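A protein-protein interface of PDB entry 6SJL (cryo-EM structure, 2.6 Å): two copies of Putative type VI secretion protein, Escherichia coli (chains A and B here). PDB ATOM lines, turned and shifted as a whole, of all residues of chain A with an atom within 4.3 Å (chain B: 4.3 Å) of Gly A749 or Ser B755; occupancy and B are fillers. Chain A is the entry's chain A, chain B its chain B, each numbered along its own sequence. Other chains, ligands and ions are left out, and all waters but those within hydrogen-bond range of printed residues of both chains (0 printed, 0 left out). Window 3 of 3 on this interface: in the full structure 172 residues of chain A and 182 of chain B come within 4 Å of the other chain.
O of Lys B754 sits at hydrogen-bond distance from N of Cys A747, 3.2 Å away.
The side-chain hydroxyl (OG) of Ser B755 lies within hydrogen-bond range of the side-chain sulfur (SG) of Cys A747.
The backbone carbonyl oxygen (O) of Cys A747 is in hydrogen-bond range of the backbone NH (N) of Thr B756.
The backbone carbonyl oxygen (O) of Gly A749 sits at hydrogen-bond distance from the side-chain hydroxyl (OG) of Ser B755 (2.8 Å).
The backbone carbonyl oxygen (O) of Gly A749 sits close to the side-chain sulfur (SG) of Cys A747, at 3.6 Å.
The backbone carbonyl oxygen (O) of Gln A750 sits at hydrogen-bond distance from the side-chain sulfur (SG) of Cys A747 (3.5 Å).
Among the printed residues, merely in contact across the chains: Gln A750 with Ser B755 (3.6 Å), Ile A751 with Leu B753 (3.96 Å) and Ile A751 with Ser B755 (3.7 Å).
Of chain A, only Cys A747 (3.4 Å), Gly A749 (2.8 Å), Gln A750 (3.6 Å) and Ile A751 (3.7 Å) come within 4 Å of Ser B755.
Of the printed residues of chain A, Thr B756 touches Cys A747 (3.4 Å).
Printed residues of chain A within 4 Å of Leu B753: Ile A751.
Pro A748 touches none of the printed residues of chain B.
The nearest printed residue of chain B that does not touch Gly A749 is Thr B756 (5.3 Å).
The nearest printed residue of chain B that does not touch Ile A751 is Lys B754 (4.5 Å).
Hydrophobic or aromatic side chains of chain A that line the printed part of chain B: Ile A751.
Along chain A the printed residues that touch a printed residue of chain B span positions 747 to 751.
Of the 4 printed residues of chain B, 4 touch a printed residue of chain A.
Printed residues of chain B that touch a printed residue of chain A: Leu B753, Lys B754, Ser B755 and Thr B756.
Hydrophobic or aromatic side chains of chain B that line the printed part of chain A: Leu B753.
Along chain B the printed residues that touch a printed residue of chain A span positions 753 to 756.
Among the printed residues, 7 pairs touch across the chains.
Among the printed residues, no Asp or Glu carboxylate lies within 4 Å of a Lys or Arg side-chain nitrogen of the other chain.
No position is printed for both chains.
Of the 7 pairs that touch across the chains among the printed residues, none has its exchanged pair printed and touching as well.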
ATOM      1  N   CYS A 747     -20.675 -10.355  16.336  1.00  0.00           N
ATOM      2  CA  CYS A 747     -20.983  -9.698  17.592  1.00  0.00           C
ATOM      3  C   CYS A 747     -22.098 -10.456  18.280  1.00  0.00           C
ATOM      4  O   CYS A 747     -22.968 -11.019  17.609  1.00  0.00           O
ATOM      5  CB  CYS A 747     -21.389  -8.234  17.399  1.00  0.00           C
ATOM      6  SG  CYS A 747     -22.949  -7.968  16.658  1.00  0.00           S
ATOM      7  N   PRO A 748     -22.081 -10.525  19.610  1.00  0.00           N
ATOM      8  CA  PRO A 748     -23.225 -11.090  20.324  1.00  0.00           C
ATOM      9  C   PRO A 748     -24.449 -10.209  20.295  1.00  0.00           C
ATOM     10  O   PRO A 748     -25.554 -10.713  20.507  1.00  0.00           O
ATOM     11  CB  PRO A 748     -22.695 -11.236  21.749  1.00  0.00           C
ATOM     12  CG  PRO A 748     -21.653 -10.211  21.845  1.00  0.00           C
ATOM     13  CD  PRO A 748     -20.997 -10.163  20.528  1.00  0.00           C
ATOM     14  N   GLY A 749     -24.294  -8.919  20.053  1.00  0.00           N
ATOM     15  CA  GLY A 749     -25.417  -8.016  20.031  1.00  0.00           C
ATOM     16  C   GLY A 749     -25.961  -7.910  18.634  1.00  0.00           C
ATOM     17  O   GLY A 749     -26.192  -8.925  17.984  1.00  0.00           O
ATOM     18  N   GLN A 750     -26.148  -6.698  18.147  1.00  0.00           N
ATOM     19  CA  GLN A 750     -26.650  -6.482  16.806  1.00  0.00           C
ATOM     20  C   GLN A 750     -25.615  -5.749  15.972  1.00  0.00           C
ATOM     21  O   GLN A 750     -24.809  -4.985  16.494  1.00  0.00           O
ATOM     22  CB  GLN A 750     -27.939  -5.685  16.834  1.00  0.00           C
ATOM     23  CG  GLN A 750     -27.728  -4.251  17.189  1.00  0.00           C
ATOM     24  CD  GLN A 750     -28.774  -3.355  16.605  1.00  0.00           C
ATOM     25  OE1 GLN A 750     -29.719  -3.814  15.969  1.00  0.00           O
ATOM     26  NE2 GLN A 750     -28.598  -2.056  16.787  1.00  0.00           N
ATOM     27  N   ILE A 751     -25.636  -5.994  14.670  1.00  0.00           N
ATOM     28  CA  ILE A 751     -24.835  -5.240  13.718  1.00  0.00           C
ATOM     29  C   ILE A 751     -25.748  -4.221  13.072  1.00  0.00           C
ATOM     30  O   ILE A 751     -26.664  -4.582  12.335  1.00  0.00           O
ATOM     31  CB  ILE A 751     -24.192  -6.149  12.667  1.00  0.00           C
ATOM     32  CG1 ILE A 751     -23.089  -6.972  13.303  1.00  0.00           C
ATOM     33  CG2 ILE A 751     -23.605  -5.332  11.591  1.00  0.00           C
ATOM     34  CD1 ILE A 751     -22.716  -8.187  12.560  1.00  0.00           C
ATOM     35  N   LEU B 753     -21.405 -11.823   8.345  1.00  0.00           N
ATOM     36  CA  LEU B 753     -21.915 -11.072   9.485  1.00  0.00           C
ATOM     37  C   LEU B 753     -22.493 -12.079  10.460  1.00  0.00           C
ATOM     38  O   LEU B 753     -23.611 -12.549  10.284  1.00  0.00           O
ATOM     39  CB  LEU B 753     -22.963 -10.054   9.078  1.00  0.00           C
ATOM     40  CG  LEU B 753     -22.662  -9.066   7.971  1.00  0.00           C
ATOM     41  CD1 LEU B 753     -23.613  -7.923   8.103  1.00  0.00           C
ATOM     42  CD2 LEU B 753     -21.278  -8.577   8.059  1.00  0.00           C
ATOM     43  N   LYS B 754     -21.719 -12.418  11.480  1.00  0.00           N
ATOM     44  CA  LYS B 754     -22.136 -13.393  12.476  1.00  0.00           C
ATOM     45  C   LYS B 754     -22.725 -12.667  13.675  1.00  0.00           C
ATOM     46  O   LYS B 754     -22.188 -12.694  14.774  1.00  0.00           O
ATOM     47  CB  LYS B 754     -20.960 -14.247  12.908  1.00  0.00           C
ATOM     48  CG  LYS B 754     -20.521 -15.266  11.943  1.00  0.00           C
ATOM     49  CD  LYS B 754     -19.244 -15.853  12.442  1.00  0.00           C
ATOM     50  CE  LYS B 754     -19.083 -17.288  12.033  1.00  0.00           C
ATOM     51  NZ  LYS B 754     -17.814 -17.838  12.557  1.00  0.00           N
ATOM     52  N   SER B 755     -23.859 -12.024  13.465  1.00  0.00           N
ATOM     53  CA  SER B 755     -24.444 -11.344  14.609  1.00  0.00           C
ATOM     54  C   SER B 755     -25.232 -12.345  15.437  1.00  0.00           C
ATOM     55  O   SER B 755     -26.408 -12.132  15.742  1.00  0.00           O
ATOM     56  CB  SER B 755     -25.322 -10.177  14.195  1.00  0.00           C
ATOM     57  OG  SER B 755     -25.955  -9.656  15.338  1.00  0.00           O
ATOM     58  N   THR B 756     -24.558 -13.445  15.779  1.00  0.00           N
ATOM     59  CA  THR B 756     -24.964 -14.421  16.785  1.00  0.00           C
ATOM     60  C   THR B 756     -23.640 -14.971  17.278  1.00  0.00           C
ATOM     61  O   THR B 756     -22.880 -15.537  16.493  1.00  0.00           O
ATOM     62  CB  THR B 756     -25.799 -15.554  16.192  1.00  0.00           C
ATOM     63  OG1 THR B 756     -25.141 -16.072  15.029  1.00  0.00           O
ATOM     64  CG2 THR B 756     -27.190 -15.103  15.852  1.00  0.00           C
